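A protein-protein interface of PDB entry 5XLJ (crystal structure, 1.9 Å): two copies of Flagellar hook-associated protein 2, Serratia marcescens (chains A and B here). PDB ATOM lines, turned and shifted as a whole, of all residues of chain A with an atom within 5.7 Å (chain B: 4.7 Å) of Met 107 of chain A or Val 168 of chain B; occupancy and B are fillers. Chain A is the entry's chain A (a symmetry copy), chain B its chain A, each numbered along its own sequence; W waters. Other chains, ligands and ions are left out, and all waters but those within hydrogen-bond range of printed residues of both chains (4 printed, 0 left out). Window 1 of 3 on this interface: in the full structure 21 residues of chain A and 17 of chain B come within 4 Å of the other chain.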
ATOM      1  N   THR A  44      27.813  28.197  -6.216  1.00  0.00           N
ATOM      2  CA  THR A  44      28.075  27.437  -4.987  1.00  0.00           C
ATOM      3  C   THR A  44      28.442  25.995  -5.287  1.00  0.00           C
ATOM      4  O   THR A  44      27.777  25.325  -6.095  1.00  0.00           O
ATOM      5  CB  THR A  44      26.869  27.503  -4.060  1.00  0.00           C
ATOM      6  OG1 THR A  44      26.490  28.882  -3.870  1.00  0.00           O
ATOM      7  CG2 THR A  44      27.163  26.805  -2.688  1.00  0.00           C
ATOM      8  N   SER A 105      33.022  32.687   0.332  1.00  0.00           N
ATOM      9  CA  SER A 105      32.690  32.388   1.718  1.00  0.00           C
ATOM     10  C   SER A 105      32.236  30.936   1.806  1.00  0.00           C
ATOM     11  O   SER A 105      31.795  30.360   0.815  1.00  0.00           O
ATOM     12  CB  SER A 105      31.601  33.327   2.238  1.00  0.00           C
ATOM     13  OG  SER A 105      30.399  33.145   1.498  1.00  0.00           O
ATOM     14  N   ILE A 106      32.336  30.352   2.996  1.00  0.00           N
ATOM     15  CA  ILE A 106      31.945  28.963   3.203  1.00  0.00           C
ATOM     16  C   ILE A 106      30.611  28.930   3.947  1.00  0.00           C
ATOM     17  O   ILE A 106      30.428  29.630   4.941  1.00  0.00           O
ATOM     18  CB  ILE A 106      33.032  28.204   3.968  1.00  0.00           C
ATOM     19  CG1 ILE A 106      34.221  28.022   3.031  1.00  0.00           C
ATOM     20  CG2 ILE A 106      32.487  26.834   4.519  1.00  0.00           C
ATOM     21  CD1 ILE A 106      35.401  27.462   3.625  1.00  0.00           C
ATOM     22  N   MET A 107      29.674  28.164   3.426  1.00  0.00           N
ATOM     23  CA  MET A 107      28.377  27.933   4.088  1.00  0.00           C
ATOM     24  C   MET A 107      28.496  26.625   4.815  1.00  0.00           C
ATOM     25  O   MET A 107      28.777  25.583   4.198  1.00  0.00           O
ATOM     26  CB  MET A 107      27.251  27.793   3.066  1.00  0.00           C
ATOM     27  CG  MET A 107      26.864  29.094   2.379  1.00  0.00           C
ATOM     28  SD  MET A 107      26.153  30.267   3.569  1.00  0.00           S
ATOM     29  CE  MET A 107      25.023  29.223   4.499  1.00  0.00           C
ATOM     30  N   ARG A 108      28.286  26.657   6.122  1.00  0.00           N
ATOM     31  CA  ARG A 108      28.204  25.430   6.869  1.00  0.00           C
ATOM     32  C   ARG A 108      26.741  25.030   6.849  1.00  0.00           C
ATOM     33  O   ARG A 108      25.916  25.574   7.602  1.00  0.00           O
ATOM     34  CB  ARG A 108      28.712  25.621   8.290  1.00  0.00           C
ATOM     35  CG  ARG A 108      28.592  24.371   9.130  1.00  0.00           C
ATOM     36  CD  ARG A 108      29.158  24.533  10.514  1.00  0.00           C
ATOM     37  NE  ARG A 108      28.783  23.376  11.323  1.00  0.00           N
ATOM     38  CZ  ARG A 108      27.602  23.204  11.916  1.00  0.00           C
ATOM     39  NH1 ARG A 108      26.661  24.133  11.862  1.00  0.00           N
ATOM     40  NH2 ARG A 108      27.359  22.084  12.591  1.00  0.00           N
ATOM     41  N   VAL A 109      26.397  24.117   5.957  1.00  0.00           N
ATOM     42  CA  VAL A 109      24.990  23.730   5.824  1.00  0.00           C
ATOM     43  C   VAL A 109      24.529  22.960   7.048  1.00  0.00           C
ATOM     44  O   VAL A 109      23.400  23.129   7.522  1.00  0.00           O
ATOM     45  CB  VAL A 109      24.751  22.963   4.498  1.00  0.00           C
ATOM     46  CG1 VAL A 109      23.303  22.462   4.379  1.00  0.00           C
ATOM     47  CG2 VAL A 109      25.109  23.877   3.321  1.00  0.00           C
ATOM     48  N   ASP A 113      28.833  19.058   6.398  1.00  0.00           N
ATOM     49  CA  ASP A 113      28.266  19.462   5.120  1.00  0.00           C
ATOM     50  C   ASP A 113      28.583  20.943   4.861  1.00  0.00           C
ATOM     51  O   ASP A 113      27.932  21.833   5.403  1.00  0.00           O
ATOM     52  CB  ASP A 113      26.762  19.190   5.151  1.00  0.00           C
ATOM     53  CG  ASP A 113      26.065  19.428   3.831  1.00  0.00           C
ATOM     54  OD1 ASP A 113      26.700  19.751   2.804  1.00  0.00           O
ATOM     55  OD2 ASP A 113      24.802  19.324   3.833  1.00  0.00           O
ATOM     56  N   TYR A 114      29.623  21.162   4.063  1.00  0.00           N
ATOM     57  CA  TYR A 114      30.136  22.484   3.745  1.00  0.00           C
ATOM     58  C   TYR A 114      30.098  22.758   2.253  1.00  0.00           C
ATOM     59  O   TYR A 114      30.333  21.853   1.438  1.00  0.00           O
ATOM     60  CB  TYR A 114      31.598  22.567   4.192  1.00  0.00           C
ATOM     61  CG  TYR A 114      31.774  22.465   5.680  1.00  0.00           C
ATOM     62  CD1 TYR A 114      31.759  23.614   6.475  1.00  0.00           C
ATOM     63  CD2 TYR A 114      31.943  21.234   6.294  1.00  0.00           C
ATOM     64  CE1 TYR A 114      31.913  23.523   7.861  1.00  0.00           C
ATOM     65  CE2 TYR A 114      32.086  21.126   7.678  1.00  0.00           C
ATOM     66  CZ  TYR A 114      32.081  22.285   8.448  1.00  0.00           C
ATOM     67  OH  TYR A 114      32.239  22.207   9.804  1.00  0.00           O
ATOM     68  N   GLN A 115      29.814  24.009   1.898  1.00  0.00           N
ATOM     69  CA  GLN A 115      29.807  24.435   0.507  1.00  0.00           C
ATOM     70  C   GLN A 115      30.542  25.765   0.375  1.00  0.00           C
ATOM     71  O   GLN A 115      30.480  26.604   1.287  1.00  0.00           O
ATOM     72  CB  GLN A 115      28.369  24.569  -0.004  1.00  0.00           C
ATOM     73  CG  GLN A 115      27.566  23.280   0.040  1.00  0.00           C
ATOM     74  CD  GLN A 115      26.110  23.468  -0.343  1.00  0.00           C
ATOM     75  OE1 GLN A 115      25.233  23.460   0.514  1.00  0.00           O
ATOM     76  NE2 GLN A 115      25.849  23.641  -1.623  1.00  0.00           N
ATOM     77  N   LEU A 116      31.225  25.957  -0.754  1.00  0.00           N
ATOM     78  CA  LEU A 116      31.945  27.181  -1.015  1.00  0.00           C
ATOM     79  C   LEU A 116      31.116  28.020  -1.983  1.00  0.00           C
ATOM     80  O   LEU A 116      30.736  27.542  -3.067  1.00  0.00           O
ATOM     81  CB  LEU A 116      33.321  26.895  -1.612  1.00  0.00           C
ATOM     82  CG  LEU A 116      34.188  28.091  -2.003  1.00  0.00           C
ATOM     83  CD1 LEU A 116      34.643  28.903  -0.779  1.00  0.00           C
ATOM     84  CD2 LEU A 116      35.417  27.565  -2.796  1.00  0.00           C
ATOM     85  N   ALA A 117      30.828  29.259  -1.593  1.00  0.00           N
ATOM     86  CA  ALA A 117      30.014  30.163  -2.423  1.00  0.00           C
ATOM     87  C   ALA A 117      30.918  31.247  -2.976  1.00  0.00           C
ATOM     88  O   ALA A 117      31.595  31.899  -2.202  1.00  0.00           O
ATOM     89  CB  ALA A 117      28.896  30.803  -1.565  1.00  0.00           C
ATOM     90  N   TYR B  30      25.400  39.739  -0.501  1.00  0.00           N
ATOM     91  CA  TYR B  30      24.532  38.639  -0.073  1.00  0.00           C
ATOM     92  C   TYR B  30      23.056  38.941  -0.323  1.00  0.00           C
ATOM     93  O   TYR B  30      22.647  40.094  -0.248  1.00  0.00           O
ATOM     94  CB  TYR B  30      24.753  38.318   1.416  1.00  0.00           C
ATOM     95  CG  TYR B  30      26.193  37.985   1.713  1.00  0.00           C
ATOM     96  CD1 TYR B  30      27.119  38.997   1.917  1.00  0.00           C
ATOM     97  CD2 TYR B  30      26.637  36.662   1.760  1.00  0.00           C
ATOM     98  CE1 TYR B  30      28.459  38.723   2.153  1.00  0.00           C
ATOM     99  CE2 TYR B  30      27.985  36.369   2.021  1.00  0.00           C
ATOM    100  CZ  TYR B  30      28.893  37.415   2.208  1.00  0.00           C
ATOM    101  OH  TYR B  30      30.245  37.171   2.440  1.00  0.00           O
ATOM    102  N   VAL B  31      22.283  37.902  -0.651  1.00  0.00           N
ATOM    103  CA  VAL B  31      20.832  37.995  -0.659  1.00  0.00           C
ATOM    104  C   VAL B  31      20.304  36.914   0.276  1.00  0.00           C
ATOM    105  O   VAL B  31      20.843  35.793   0.322  1.00  0.00           O
ATOM    106  CB  VAL B  31      20.211  37.916  -2.097  1.00  0.00           C
ATOM    107  CG1 VAL B  31      20.692  39.115  -2.964  1.00  0.00           C
ATOM    108  CG2 VAL B  31      20.583  36.623  -2.791  1.00  0.00           C
ATOM    109  N   LEU B 166      15.913  29.291   5.997  1.00  0.00           N
ATOM    110  CA  LEU B 166      16.324  30.477   5.261  1.00  0.00           C
ATOM    111  C   LEU B 166      17.238  30.076   4.123  1.00  0.00           C
ATOM    112  O   LEU B 166      17.743  28.952   4.084  1.00  0.00           O
ATOM    113  CB  LEU B 166      17.016  31.490   6.167  1.00  0.00           C
ATOM    114  CG  LEU B 166      18.349  31.150   6.818  1.00  0.00           C
ATOM    115  CD1 LEU B 166      19.116  32.427   7.126  1.00  0.00           C
ATOM    116  CD2 LEU B 166      18.120  30.308   8.092  1.00  0.00           C
ATOM    117  N   THR B 167      17.434  30.987   3.185  1.00  0.00           N
ATOM    118  CA  THR B 167      18.433  30.768   2.159  1.00  0.00           C
ATOM    119  C   THR B 167      19.424  31.914   2.200  1.00  0.00           C
ATOM    120  O   THR B 167      19.037  33.070   2.350  1.00  0.00           O
ATOM    121  CB  THR B 167      17.790  30.619   0.775  1.00  0.00           C
ATOM    122  OG1 THR B 167      17.295  31.891   0.340  1.00  0.00           O
ATOM    123  CG2 THR B 167      16.666  29.626   0.840  1.00  0.00           C
ATOM    124  N   VAL B 168      20.706  31.578   2.102  1.00  0.00           N
ATOM    125  CA  VAL B 168      21.759  32.560   2.048  1.00  0.00           C
ATOM    126  C   VAL B 168      22.481  32.392   0.730  1.00  0.00           C
ATOM    127  O   VAL B 168      23.037  31.326   0.457  1.00  0.00           O
ATOM    128  CB  VAL B 168      22.777  32.371   3.169  1.00  0.00           C
ATOM    129  CG1 VAL B 168      23.878  33.451   3.066  1.00  0.00           C
ATOM    130  CG2 VAL B 168      22.068  32.374   4.533  1.00  0.00           C
ATOM    131  N   ASN B 169      22.445  33.451  -0.080  1.00  0.00           N
ATOM    132  CA  ASN B 169      22.901  33.412  -1.463  1.00  0.00           C
ATOM    133  C   ASN B 169      22.479  32.117  -2.153  1.00  0.00           C
ATOM    134  O   ASN B 169      23.272  31.432  -2.795  1.00  0.00           O
ATOM    135  CB  ASN B 169      24.409  33.644  -1.551  1.00  0.00           C
ATOM    136  CG  ASN B 169      24.778  35.128  -1.703  1.00  0.00           C
ATOM    137  OD1 ASN B 169      23.958  35.965  -2.099  1.00  0.00           O
ATOM    138  ND2 ASN B 169      26.035  35.444  -1.433  1.00  0.00           N
ATOM    139  N   GLY B 170      21.196  31.791  -1.980  1.00  0.00           N
ATOM    140  CA  GLY B 170      20.578  30.682  -2.665  1.00  0.00           C
ATOM    141  C   GLY B 170      20.801  29.304  -2.074  1.00  0.00           C
ATOM    142  O   GLY B 170      20.333  28.336  -2.650  1.00  0.00           O
ATOM    143  N   THR B 171      21.521  29.205  -0.948  1.00  0.00           N
ATOM    144  CA  THR B 171      21.746  27.918  -0.252  1.00  0.00           C
ATOM    145  C   THR B 171      20.849  27.839   0.971  1.00  0.00           C
ATOM    146  O   THR B 171      20.899  28.709   1.856  1.00  0.00           O
ATOM    147  CB  THR B 171      23.221  27.745   0.154  1.00  0.00           C
ATOM    148  OG1 THR B 171      24.027  27.709  -1.030  1.00  0.00           O
ATOM    149  CG2 THR B 171      23.451  26.448   0.959  1.00  0.00           C
ATOM    150  N   ILE B 173      19.309  26.608   4.419  1.00  0.00           N
ATOM    151  CA  ILE B 173      19.843  26.339   5.754  1.00  0.00           C
ATOM    152  C   ILE B 173      18.608  26.085   6.638  1.00  0.00           C
ATOM    153  O   ILE B 173      17.604  26.807   6.510  1.00  0.00           O
ATOM    154  CB  ILE B 173      20.556  27.615   6.304  1.00  0.00           C
ATOM    155  CG1 ILE B 173      21.829  27.931   5.501  1.00  0.00           C
ATOM    156  CG2 ILE B 173      20.949  27.455   7.777  1.00  0.00           C
ATOM    157  CD1 ILE B 173      22.799  26.745   5.451  1.00  0.00           C
ATOM    158  N   ALA B 183      26.328  29.130  10.384  1.00  0.00           N
ATOM    159  CA  ALA B 183      26.087  28.914   8.963  1.00  0.00           C
ATOM    160  C   ALA B 183      27.157  29.631   8.135  1.00  0.00           C
ATOM    161  O   ALA B 183      27.863  29.030   7.344  1.00  0.00           O
ATOM    162  CB  ALA B 183      24.676  29.414   8.598  1.00  0.00           C
ATOM    163  N   LEU B 184      27.306  30.928   8.365  1.00  0.00           N
ATOM    164  CA  LEU B 184      28.291  31.762   7.612  1.00  0.00           C
ATOM    165  C   LEU B 184      29.316  32.248   8.636  1.00  0.00           C
ATOM    166  O   LEU B 184      28.933  32.824   9.663  1.00  0.00           O
ATOM    167  CB  LEU B 184      27.496  32.867   6.889  1.00  0.00           C
ATOM    168  CG  LEU B 184      28.025  33.867   5.847  1.00  0.00           C
ATOM    169  CD1 LEU B 184      28.517  33.174   4.559  1.00  0.00           C
ATOM    170  CD2 LEU B 184      26.913  34.864   5.533  1.00  0.00           C
ATOM    171  N   ILE B 189      22.923  35.691  12.048  1.00  0.00           N
ATOM    172  CA  ILE B 189      21.692  36.191  11.474  1.00  0.00           C
ATOM    173  C   ILE B 189      20.590  35.919  12.483  1.00  0.00           C
ATOM    174  O   ILE B 189      20.260  34.754  12.742  1.00  0.00           O
ATOM    175  CB  ILE B 189      21.340  35.465  10.178  1.00  0.00           C
ATOM    176  CG1 ILE B 189      22.510  35.561   9.194  1.00  0.00           C
ATOM    177  CG2 ILE B 189      20.049  36.047   9.578  1.00  0.00           C
ATOM    178  CD1 ILE B 189      22.271  34.829   7.867  1.00  0.00           C
HETATM  179  O   HOH W   1      25.333  29.890  -1.624  1.00  0.00           O
HETATM  180  O   HOH W   2      27.543  33.820   0.007  1.00  0.00           O
HETATM  181  O   HOH W   3      23.814  25.377  -2.667  1.00  0.00           O
HETATM  182  O   HOH W   4      26.319  31.536   0.574  1.00  0.00           O
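O of Ala 183 of chain B sits at hydrogen-bond distance from N of Arg 108 of chain A, at 2.7 Å.
The backbone carbonyl oxygen (O) of Leu 166 of chain B sits at hydrogen-bond distance from the backbone NH (N) of Ile 173 of chain B (2.8 Å).
The backbone NH of Ala 117 of chain A sits at hydrogen-bond distance from the backbone carbonyl oxygen of Ser 105 of chain A (2.8 Å).
The backbone NH (N) of Met 107 of chain A sits at hydrogen-bond distance from the backbone carbonyl oxygen (O) of Gln 115 of chain A (2.8 Å).
OG1 of Thr 171 of chain B touches CG2 of Thr 44 of chain A, at 3.7 Å.
CD1 of Leu 184 of chain B touches OG of Ser 105 of chain A, at 3.6 Å.
Ala 183 of chain B touches Ile 106 of chain A.
CG1 of Val 168 of chain B touches SD of Met 107 of chain A, 3.9 Å away.
Ile 173 of chain B touches Met 107 of chain A (CD1 to CE, 3.5 Å).
Ala 183 of chain B touches Met 107 of chain A (O to CA, 3.5 Å).
Met 107 of chain A touches Leu 184 of chain B (SD to CD1, 3.9 Å).
Ile 173 of chain B touches Arg 108 of chain A.
CG2 of Thr 171 of chain B touches CG2 of Val 109 of chain A, at 3.9 Å.
Ile 173 of chain B touches Val 109 of chain A.
Of the printed residues of chain B, Met 107 of chain A touches Val 168, Ile 173, Ala 183 and Leu 184.
Of chain A, only Met 107 (3.9 Å) comes within 4 Å of Val 168 of chain B.
Printed residues of chain B within 4 Å of Ser 105 of chain A: Leu 184 (3.6 Å).
Printed residues of chain B within 4 Å of Ile 106 of chain A: Ala 183 (3.6 Å).
Of the printed residues of chain B, Gln 115 of chain A touches Thr 171 (3.5 Å).
Of the printed residues of chain B, Val 109 of chain A touches Thr 171 (3.9 Å) and Ile 173 (3.7 Å).
Asp 113 of chain A touches none of the printed residues of chain B.
The nearest residue of chain B that does not touch Met 107 of chain A is Thr 171 of chain B (4.5 Å).
The nearest printed residue of chain A that does not touch Val 168 of chain B is Thr 44 of chain A (6.1 Å).
The nearest printed residue of chain A that does not touch Ile 173 of chain B is Gln 115 of chain A (6.4 Å).
Hydrophobic or aromatic side chains of chain A within 4 Å of the printed part of chain B: Met 107 and Val 109.
Of the 12 printed residues of chain B, 5 touch a printed residue of chain A.
Printed residues of chain B that touch a printed residue of chain A: Val 168, Thr 171, Ile 173, Ala 183 and Leu 184.
Hydrophobic or aromatic side chains of chain B that line the printed part of chain A: Val 168, Ile 173 and Leu 184.
Among the printed residues, 12 pairs touch across the chains.
Among the printed residues, no Asp or Glu carboxylate lies within 4 Å of a Lys or Arg side-chain nitrogen of the other chain.
No position is printed for both chains.
Water W1 lies within hydrogen-bond range of the side-chain hydroxyl of Thr 171 of chain B, the side-chain hydroxyl of Thr 44 of chain A, the backbone carbonyl oxygen of Asn 169 of chain B and the backbone carbonyl oxygen of Val 168 of chain B.
Water W2 bridges the side-chain amide nitrogen (ND2) of Asn 169 of chain B and the side-chain hydroxyl (OG) of Ser 105 of chain A.
Water W3 lies within hydrogen-bond range of the side-chain hydroxyl (OG1) of Thr 171 of chain B and the side-chain amide nitrogen (NE2) of Gln 115 of chain A.
Water W4 lies within hydrogen-bond range of SD of Met 107 of chain A (3.3 Å) and O of Val 168 of chain B (3.3 Å).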
